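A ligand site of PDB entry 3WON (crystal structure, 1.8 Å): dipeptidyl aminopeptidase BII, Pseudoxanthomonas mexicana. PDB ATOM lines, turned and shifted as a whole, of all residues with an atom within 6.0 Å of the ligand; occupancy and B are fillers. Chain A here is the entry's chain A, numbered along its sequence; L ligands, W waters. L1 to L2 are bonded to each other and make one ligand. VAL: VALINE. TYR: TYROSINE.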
ATOM      1  N   GLY A  45      19.139  21.002   8.058  1.00  0.00           N
ATOM      2  CA  GLY A  45      18.891  21.836   6.926  1.00  0.00           C
ATOM      3  C   GLY A  45      20.017  21.929   5.856  1.00  0.00           C
ATOM      4  O   GLY A  45      19.834  22.571   4.784  1.00  0.00           O
ATOM      5  N   CYS A  46      21.135  21.271   6.094  1.00  0.00           N
ATOM      6  CA  CYS A  46      22.146  21.002   5.054  1.00  0.00           C
ATOM      7  C   CYS A  46      22.638  19.551   5.242  1.00  0.00           C
ATOM      8  O   CYS A  46      22.420  18.955   6.279  1.00  0.00           O
ATOM      9  CB  CYS A  46      23.348  21.993   5.227  1.00  0.00           C
ATOM     10  SG  CYS A  46      23.141  23.585   4.220  1.00  0.00           S
ATOM     11  N   ASN A  60      28.994  22.858   2.040  1.00  0.00           N
ATOM     12  CA  ASN A  60      29.044  24.032   1.243  1.00  0.00           C
ATOM     13  C   ASN A  60      29.401  25.221   2.109  1.00  0.00           C
ATOM     14  O   ASN A  60      29.081  25.224   3.303  1.00  0.00           O
ATOM     15  CB  ASN A  60      27.702  24.334   0.588  1.00  0.00           C
ATOM     16  CG  ASN A  60      27.318  23.379  -0.498  1.00  0.00           C
ATOM     17  OD1 ASN A  60      28.111  22.669  -1.185  1.00  0.00           O
ATOM     18  ND2 ASN A  60      26.102  23.435  -0.752  1.00  0.00           N
ATOM     19  N   HIS A  62      27.892  28.075   1.674  1.00  0.00           N
ATOM     20  CA  HIS A  62      26.629  28.690   2.092  1.00  0.00           C
ATOM     21  C   HIS A  62      25.998  27.947   3.292  1.00  0.00           C
ATOM     22  O   HIS A  62      25.215  28.531   4.038  1.00  0.00           O
ATOM     23  CB  HIS A  62      25.669  28.924   0.918  1.00  0.00           C
ATOM     24  CG  HIS A  62      24.934  27.719   0.467  1.00  0.00           C
ATOM     25  ND1 HIS A  62      25.382  26.950  -0.572  1.00  0.00           N
ATOM     26  CD2 HIS A  62      23.801  27.143   0.910  1.00  0.00           C
ATOM     27  CE1 HIS A  62      24.528  25.976  -0.802  1.00  0.00           C
ATOM     28  NE2 HIS A  62      23.587  26.034   0.117  1.00  0.00           N
ATOM     29  N   CYS A  63      26.338  26.670   3.493  1.00  0.00           N
ATOM     30  CA  CYS A  63      25.921  25.963   4.694  1.00  0.00           C
ATOM     31  C   CYS A  63      26.680  26.426   5.916  1.00  0.00           C
ATOM     32  O   CYS A  63      26.134  26.378   7.022  1.00  0.00           O
ATOM     33  CB  CYS A  63      26.101  24.446   4.512  1.00  0.00           C
ATOM     34  SG  CYS A  63      25.075  23.835   3.159  1.00  0.00           S
ATOM     35  N   ASN A 191      23.220  33.123  -8.325  1.00  0.00           N
ATOM     36  CA  ASN A 191      22.351  32.209  -7.596  1.00  0.00           C
ATOM     37  C   ASN A 191      21.186  31.703  -8.427  1.00  0.00           C
ATOM     38  O   ASN A 191      20.555  32.497  -9.150  1.00  0.00           O
ATOM     39  CB  ASN A 191      21.827  32.918  -6.333  1.00  0.00           C
ATOM     40  CG  ASN A 191      21.275  31.960  -5.304  1.00  0.00           C
ATOM     41  OD1 ASN A 191      21.673  30.747  -5.233  1.00  0.00           O
ATOM     42  ND2 ASN A 191      20.315  32.442  -4.526  1.00  0.00           N
ATOM     43  N   TRP A 192      20.909  30.392  -8.340  1.00  0.00           N
ATOM     44  CA  TRP A 192      19.928  29.692  -9.137  1.00  0.00           C
ATOM     45  C   TRP A 192      20.264  29.725 -10.599  1.00  0.00           C
ATOM     46  O   TRP A 192      19.380  29.538 -11.400  1.00  0.00           O
ATOM     47  CB  TRP A 192      18.522  30.194  -8.934  1.00  0.00           C
ATOM     48  CG  TRP A 192      18.076  30.096  -7.525  1.00  0.00           C
ATOM     49  CD1 TRP A 192      17.896  31.155  -6.651  1.00  0.00           C
ATOM     50  CD2 TRP A 192      17.804  28.926  -6.783  1.00  0.00           C
ATOM     51  NE1 TRP A 192      17.460  30.686  -5.428  1.00  0.00           N
ATOM     52  CE2 TRP A 192      17.404  29.322  -5.481  1.00  0.00           C
ATOM     53  CE3 TRP A 192      17.821  27.575  -7.085  1.00  0.00           C
ATOM     54  CZ2 TRP A 192      17.090  28.393  -4.479  1.00  0.00           C
ATOM     55  CZ3 TRP A 192      17.489  26.671  -6.086  1.00  0.00           C
ATOM     56  CH2 TRP A 192      17.183  27.072  -4.784  1.00  0.00           C
ATOM     57  N   ARG A 196      27.742  28.486 -13.924  1.00  0.00           N
ATOM     58  CA  ARG A 196      27.972  28.811 -12.558  1.00  0.00           C
ATOM     59  C   ARG A 196      29.499  28.603 -12.347  1.00  0.00           C
ATOM     60  O   ARG A 196      30.116  27.617 -12.901  1.00  0.00           O
ATOM     61  CB  ARG A 196      27.193  27.884 -11.604  1.00  0.00           C
ATOM     62  CG  ARG A 196      27.141  28.399 -10.180  1.00  0.00           C
ATOM     63  CD  ARG A 196      26.558  29.763 -10.055  1.00  0.00           C
ATOM     64  NE  ARG A 196      26.104  29.910  -8.658  1.00  0.00           N
ATOM     65  CZ  ARG A 196      24.980  29.387  -8.195  1.00  0.00           C
ATOM     66  NH1 ARG A 196      24.149  28.711  -9.033  1.00  0.00           N
ATOM     67  NH2 ARG A 196      24.677  29.513  -6.894  1.00  0.00           N
ATOM     68  N   ASP A 200      31.724  26.633  -3.822  1.00  0.00           N
ATOM     69  CA  ASP A 200      30.845  26.571  -2.653  1.00  0.00           C
ATOM     70  C   ASP A 200      31.170  25.365  -1.749  1.00  0.00           C
ATOM     71  O   ASP A 200      30.528  24.306  -1.778  1.00  0.00           O
ATOM     72  CB  ASP A 200      29.390  26.520  -3.155  1.00  0.00           C
ATOM     73  CG  ASP A 200      28.425  26.989  -2.091  1.00  0.00           C
ATOM     74  OD1 ASP A 200      28.845  27.092  -0.918  1.00  0.00           O
ATOM     75  OD2 ASP A 200      27.261  27.230  -2.440  1.00  0.00           O
ATOM     76  N   ASN A 306      17.894  34.346  -1.310  1.00  0.00           N
ATOM     77  CA  ASN A 306      17.820  32.997  -1.906  1.00  0.00           C
ATOM     78  C   ASN A 306      16.363  32.537  -2.092  1.00  0.00           C
ATOM     79  O   ASN A 306      15.946  32.078  -3.164  1.00  0.00           O
ATOM     80  CB  ASN A 306      18.575  32.051  -1.025  1.00  0.00           C
ATOM     81  CG  ASN A 306      18.663  30.644  -1.638  1.00  0.00           C
ATOM     82  OD1 ASN A 306      19.069  30.499  -2.777  1.00  0.00           O
ATOM     83  ND2 ASN A 306      18.297  29.668  -0.899  1.00  0.00           N
ATOM     84  N   ASN A 310      14.280  32.163  -5.563  1.00  0.00           N
ATOM     85  CA  ASN A 310      13.744  30.875  -5.812  1.00  0.00           C
ATOM     86  C   ASN A 310      12.283  31.007  -6.224  1.00  0.00           C
ATOM     87  O   ASN A 310      11.816  30.401  -7.166  1.00  0.00           O
ATOM     88  CB  ASN A 310      13.774  29.986  -4.571  1.00  0.00           C
ATOM     89  CG  ASN A 310      13.181  28.617  -4.832  1.00  0.00           C
ATOM     90  OD1 ASN A 310      13.862  27.637  -5.275  1.00  0.00           O
ATOM     91  ND2 ASN A 310      11.991  28.535  -4.694  1.00  0.00           N
ATOM     92  N   ILE A 628      17.485  16.921  -6.684  1.00  0.00           N
ATOM     93  CA  ILE A 628      17.767  17.429  -5.359  1.00  0.00           C
ATOM     94  C   ILE A 628      16.943  18.666  -5.102  1.00  0.00           C
ATOM     95  O   ILE A 628      16.362  19.254  -6.009  1.00  0.00           O
ATOM     96  CB  ILE A 628      19.229  17.756  -5.145  1.00  0.00           C
ATOM     97  CG1 ILE A 628      19.807  18.740  -6.175  1.00  0.00           C
ATOM     98  CG2 ILE A 628      20.032  16.476  -5.221  1.00  0.00           C
ATOM     99  CD1 ILE A 628      21.105  19.395  -5.625  1.00  0.00           C
ATOM    100  N   THR A 629      16.941  19.063  -3.842  1.00  0.00           N
ATOM    101  CA  THR A 629      16.284  20.299  -3.453  1.00  0.00           C
ATOM    102  C   THR A 629      16.842  20.864  -2.174  1.00  0.00           C
ATOM    103  O   THR A 629      17.780  20.285  -1.605  1.00  0.00           O
ATOM    104  CB  THR A 629      14.744  20.103  -3.454  1.00  0.00           C
ATOM    105  OG1 THR A 629      14.154  21.407  -3.370  1.00  0.00           O
ATOM    106  CG2 THR A 629      14.271  19.341  -2.301  1.00  0.00           C
ATOM    107  N   GLY A 630      16.232  21.927  -1.658  1.00  0.00           N
ATOM    108  CA  GLY A 630      16.652  22.546  -0.390  1.00  0.00           C
ATOM    109  C   GLY A 630      16.895  21.506   0.713  1.00  0.00           C
ATOM    110  O   GLY A 630      16.058  20.633   0.933  1.00  0.00           O
ATOM    111  N   GLY A 631      18.031  21.560   1.367  1.00  0.00           N
ATOM    112  CA  GLY A 631      18.457  20.555   2.333  1.00  0.00           C
ATOM    113  C   GLY A 631      19.575  19.652   1.777  1.00  0.00           C
ATOM    114  O   GLY A 631      20.403  19.143   2.538  1.00  0.00           O
ATOM    115  N   ASN A 632      19.636  19.512   0.454  1.00  0.00           N
ATOM    116  CA  ASN A 632      20.708  18.776  -0.213  1.00  0.00           C
ATOM    117  C   ASN A 632      21.995  19.549  -0.393  1.00  0.00           C
ATOM    118  O   ASN A 632      22.983  18.934  -0.772  1.00  0.00           O
ATOM    119  CB  ASN A 632      20.273  18.255  -1.608  1.00  0.00           C
ATOM    120  CG  ASN A 632      19.701  16.888  -1.575  1.00  0.00           C
ATOM    121  OD1 ASN A 632      20.401  15.886  -1.159  1.00  0.00           O
ATOM    122  ND2 ASN A 632      18.504  16.762  -2.052  1.00  0.00           N
ATOM    123  N   SER A 633      22.045  20.842  -0.125  1.00  0.00           N
ATOM    124  CA  SER A 633      23.300  21.551  -0.195  1.00  0.00           C
ATOM    125  C   SER A 633      24.298  20.896   0.734  1.00  0.00           C
ATOM    126  O   SER A 633      23.899  20.446   1.815  1.00  0.00           O
ATOM    127  CB  SER A 633      23.115  23.003   0.209  1.00  0.00           C
ATOM    128  OG  SER A 633      22.777  23.643  -1.020  1.00  0.00           O
ATOM    129  N   PHE A 649      25.296  21.802  -4.635  1.00  0.00           N
ATOM    130  CA  PHE A 649      24.936  23.123  -4.033  1.00  0.00           C
ATOM    131  C   PHE A 649      23.777  23.893  -4.572  1.00  0.00           C
ATOM    132  O   PHE A 649      23.295  24.768  -3.831  1.00  0.00           O
ATOM    133  CB  PHE A 649      26.182  24.057  -3.850  1.00  0.00           C
ATOM    134  CG  PHE A 649      26.721  24.688  -5.136  1.00  0.00           C
ATOM    135  CD1 PHE A 649      27.591  24.008  -5.995  1.00  0.00           C
ATOM    136  CD2 PHE A 649      26.423  26.004  -5.456  1.00  0.00           C
ATOM    137  CE1 PHE A 649      28.132  24.586  -7.133  1.00  0.00           C
ATOM    138  CE2 PHE A 649      26.965  26.593  -6.604  1.00  0.00           C
ATOM    139  CZ  PHE A 649      27.842  25.895  -7.450  1.00  0.00           C
ATOM    140  N   ASP A 650      23.309  23.704  -5.809  1.00  0.00           N
ATOM    141  CA  ASP A 650      22.248  24.560  -6.350  1.00  0.00           C
ATOM    142  C   ASP A 650      21.556  23.780  -7.464  1.00  0.00           C
ATOM    143  O   ASP A 650      21.897  22.623  -7.764  1.00  0.00           O
ATOM    144  CB  ASP A 650      22.819  25.869  -6.869  1.00  0.00           C
ATOM    145  CG  ASP A 650      21.816  27.065  -6.797  1.00  0.00           C
ATOM    146  OD1 ASP A 650      20.598  26.832  -6.466  1.00  0.00           O
ATOM    147  OD2 ASP A 650      22.238  28.150  -7.142  1.00  0.00           O
ATOM    148  N   GLY A 651      20.509  24.413  -7.985  1.00  0.00           N
ATOM    149  CA  GLY A 651      19.898  24.044  -9.227  1.00  0.00           C
ATOM    150  C   GLY A 651      19.856  25.145 -10.231  1.00  0.00           C
ATOM    151  O   GLY A 651      19.957  26.337  -9.881  1.00  0.00           O
ATOM    152  N   ASN A 652      19.709  24.775 -11.502  1.00  0.00           N
ATOM    153  CA  ASN A 652      19.617  25.753 -12.526  1.00  0.00           C
ATOM    154  C   ASN A 652      18.231  26.427 -12.492  1.00  0.00           C
ATOM    155  O   ASN A 652      17.336  25.907 -11.864  1.00  0.00           O
ATOM    156  CB  ASN A 652      19.848  25.067 -13.868  1.00  0.00           C
ATOM    157  CG  ASN A 652      18.864  23.964 -14.120  1.00  0.00           C
ATOM    158  OD1 ASN A 652      18.882  22.934 -13.467  1.00  0.00           O
ATOM    159  ND2 ASN A 652      17.962  24.177 -15.081  1.00  0.00           N
ATOM    160  N   SER A 655      14.961  24.676 -13.145  1.00  0.00           N
ATOM    161  CA  SER A 655      14.755  23.488 -12.364  1.00  0.00           C
ATOM    162  C   SER A 655      13.750  23.686 -11.243  1.00  0.00           C
ATOM    163  O   SER A 655      13.261  22.707 -10.694  1.00  0.00           O
ATOM    164  CB  SER A 655      16.064  22.964 -11.771  1.00  0.00           C
ATOM    165  OG  SER A 655      16.526  23.693 -10.600  1.00  0.00           O
ATOM    166  N   VAL A 656      13.604  24.925 -10.795  1.00  0.00           N
ATOM    167  CA  VAL A 656      13.106  25.156  -9.389  1.00  0.00           C
ATOM    168  C   VAL A 656      11.586  24.830  -9.303  1.00  0.00           C
ATOM    169  O   VAL A 656      11.083  24.356  -8.270  1.00  0.00           O
ATOM    170  CB  VAL A 656      13.432  26.547  -8.849  1.00  0.00           C
ATOM    171  CG1 VAL A 656      14.931  26.682  -8.633  1.00  0.00           C
ATOM    172  CG2 VAL A 656      12.919  27.707  -9.710  1.00  0.00           C
ATOM    173  N   ARG A 668      18.320  20.116 -13.433  1.00  0.00           N
ATOM    174  CA  ARG A 668      19.698  19.671 -13.153  1.00  0.00           C
ATOM    175  C   ARG A 668      20.192  20.118 -11.778  1.00  0.00           C
ATOM    176  O   ARG A 668      19.792  21.183 -11.313  1.00  0.00           O
ATOM    177  CB  ARG A 668      20.594  20.282 -14.195  1.00  0.00           C
ATOM    178  CG  ARG A 668      20.354  19.875 -15.662  1.00  0.00           C
ATOM    179  CD  ARG A 668      20.656  18.434 -15.933  1.00  0.00           C
ATOM    180  NE  ARG A 668      20.396  18.087 -17.340  1.00  0.00           N
ATOM    181  CZ  ARG A 668      19.266  17.583 -17.817  1.00  0.00           C
ATOM    182  NH1 ARG A 668      18.231  17.415 -17.046  1.00  0.00           N
ATOM    183  NH2 ARG A 668      19.162  17.333 -19.117  1.00  0.00           N
ATOM    184  N   MET A 669      21.044  19.313 -11.177  1.00  0.00           N
ATOM    185  CA  MET A 669      21.906  19.684 -10.061  1.00  0.00           C
ATOM    186  C   MET A 669      23.102  20.450 -10.580  1.00  0.00           C
ATOM    187  O   MET A 669      23.673  20.073 -11.612  1.00  0.00           O
ATOM    188  CB  MET A 669      22.396  18.444  -9.300  1.00  0.00           C
ATOM    189  CG  MET A 669      23.569  18.677  -8.368  1.00  0.00           C
ATOM    190  SD  MET A 669      23.985  17.314  -7.282  1.00  0.00           S
ATOM    191  CE  MET A 669      24.947  16.330  -8.518  1.00  0.00           C
HETATM  192  N   VAL L   1      20.544  28.478  -4.280  1.00  0.00           N
HETATM  193  CA  VAL L   1      21.284  27.487  -3.478  1.00  0.00           C
HETATM  194  C   VAL L   1      20.329  26.676  -2.628  1.00  0.00           C
HETATM  195  O   VAL L   1      19.239  27.140  -2.195  1.00  0.00           O
HETATM  196  CB  VAL L   1      22.459  28.073  -2.661  1.00  0.00           C
HETATM  197  CG1 VAL L   1      23.593  28.585  -3.574  1.00  0.00           C
HETATM  198  CG2 VAL L   1      21.965  29.133  -1.648  1.00  0.00           C
HETATM  199  N   TYR L   2      20.668  25.426  -2.461  1.00  0.00           N
HETATM  200  CA  TYR L   2      19.818  24.529  -1.711  1.00  0.00           C
HETATM  201  C   TYR L   2      20.218  24.428  -0.264  1.00  0.00           C
HETATM  202  O   TYR L   2      20.080  23.356   0.329  1.00  0.00           O
HETATM  203  CB  TYR L   2      19.933  23.140  -2.423  1.00  0.00           C
HETATM  204  CG  TYR L   2      19.126  23.051  -3.659  1.00  0.00           C
HETATM  205  CD1 TYR L   2      17.858  23.537  -3.737  1.00  0.00           C
HETATM  206  CD2 TYR L   2      19.662  22.457  -4.848  1.00  0.00           C
HETATM  207  CE1 TYR L   2      17.100  23.392  -4.915  1.00  0.00           C
HETATM  208  CE2 TYR L   2      18.930  22.358  -5.990  1.00  0.00           C
HETATM  209  CZ  TYR L   2      17.664  22.799  -6.045  1.00  0.00           C
HETATM  210  OH  TYR L   2      16.913  22.683  -7.209  1.00  0.00           O
HETATM  211  OXT TYR L   2      20.792  25.361   0.325  1.00  0.00           O
HETATM  212  O   HOH W   1      13.881  22.400  -6.202  1.00  0.00           O
HETATM  213  O   HOH W   2      20.307  24.879   2.795  1.00  0.00           O
HETATM  214  O   HOH W   3      18.182  20.979  -9.087  1.00  0.00           O
HETATM  215  O   HOH W   4      16.585  26.513  -1.340  1.00  0.00           O
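CH2 of Trp 192 touches O of VAL L1 (3.3 Å). NH2 of Arg 196 touches CG1 of VAL L1, at 3.6 Å. CD1 of Ile 628 touches CD2 of TYR L2, at 3.5 Å. C of Thr 629 touches CD1 of TYR L2 (3.3 Å). Gly 630 touches the ligand. Asn 632 touches the ligand. N of Gly 651 touches CE2 of TYR L2 (3.3 Å). OG of Ser 655 touches OH of TYR L2 (3.6 Å). The nearest printed residue that does not touch the ligand is Asp 200 (4.1 Å).
The side-chain amide oxygen of Asn 191 is in hydrogen-bond range of a nitrogen (N) of VAL L1 (2.7 Å). The side-chain carboxylate (OD1) of Asp 650 lies within salt-bridge range of a nitrogen (N) of VAL L1 (2.7 Å). An oxygen (O) of TYR L2 sits close to the backbone NH of Ser 633 (3.2 Å). An oxygen (OXT) of TYR L2 lies close to the side-chain hydroxyl (OG) of Ser 633, at 2.9 Å. A ring nitrogen (NE2) of His 62 lies within hydrogen-bond range of an oxygen (OXT) of TYR L2 (2.9 Å). The backbone NH (N) of Gly 631 is in hydrogen-bond range of an oxygen (O) of TYR L2 (2.9 Å). OD1 of Asn 306 sits at hydrogen-bond distance from N of VAL L1. O of Phe 649 is in hydrogen-bond range of N of TYR L2, at 3.0 Å.
The side-chain amide nitrogen of Asn 191 sits close to the indole nitrogen of Trp 192, 3.5 Å away. The side-chain carboxylate (OD2) of Asp 650 lies within salt-bridge range of the guanidinium group (NH1) of Arg 196 (2.7 Å). The side-chain hydroxyl (OG) of Ser 633 sits at hydrogen-bond distance from the backbone carbonyl oxygen (O) of Phe 649. The side-chain hydroxyl (OG) of Ser 633 sits close to the side-chain amide nitrogen (ND2) of Asn 60. A ring nitrogen (ND1) of His 62 sits at hydrogen-bond distance from the side-chain carboxylate (OD2) of Asp 200. The backbone NH of Thr 629 sits close to the side-chain amide nitrogen of Asn 632 (3.3 Å). OG of Ser 655 is in hydrogen-bond range of O of Asn 652 (2.7 Å). The side-chain sulfur (SG) of Cys 63 forms a disulfide with the side-chain sulfur (SG) of Cys 46 (2.2 Å).
Water W2 lies within hydrogen-bond range of OXT of TYR L2 (2.6 Å), O of Gly 45 (3.1 Å) and SG of Cys 46 (3.4 Å). Water W3 bridges O of Arg 668 and OH of TYR L2. Water W1 lies within hydrogen-bond range of the side-chain hydroxyl of Thr 629 (3.0 Å) and an oxygen (OH) of TYR L2 (3.2 Å).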
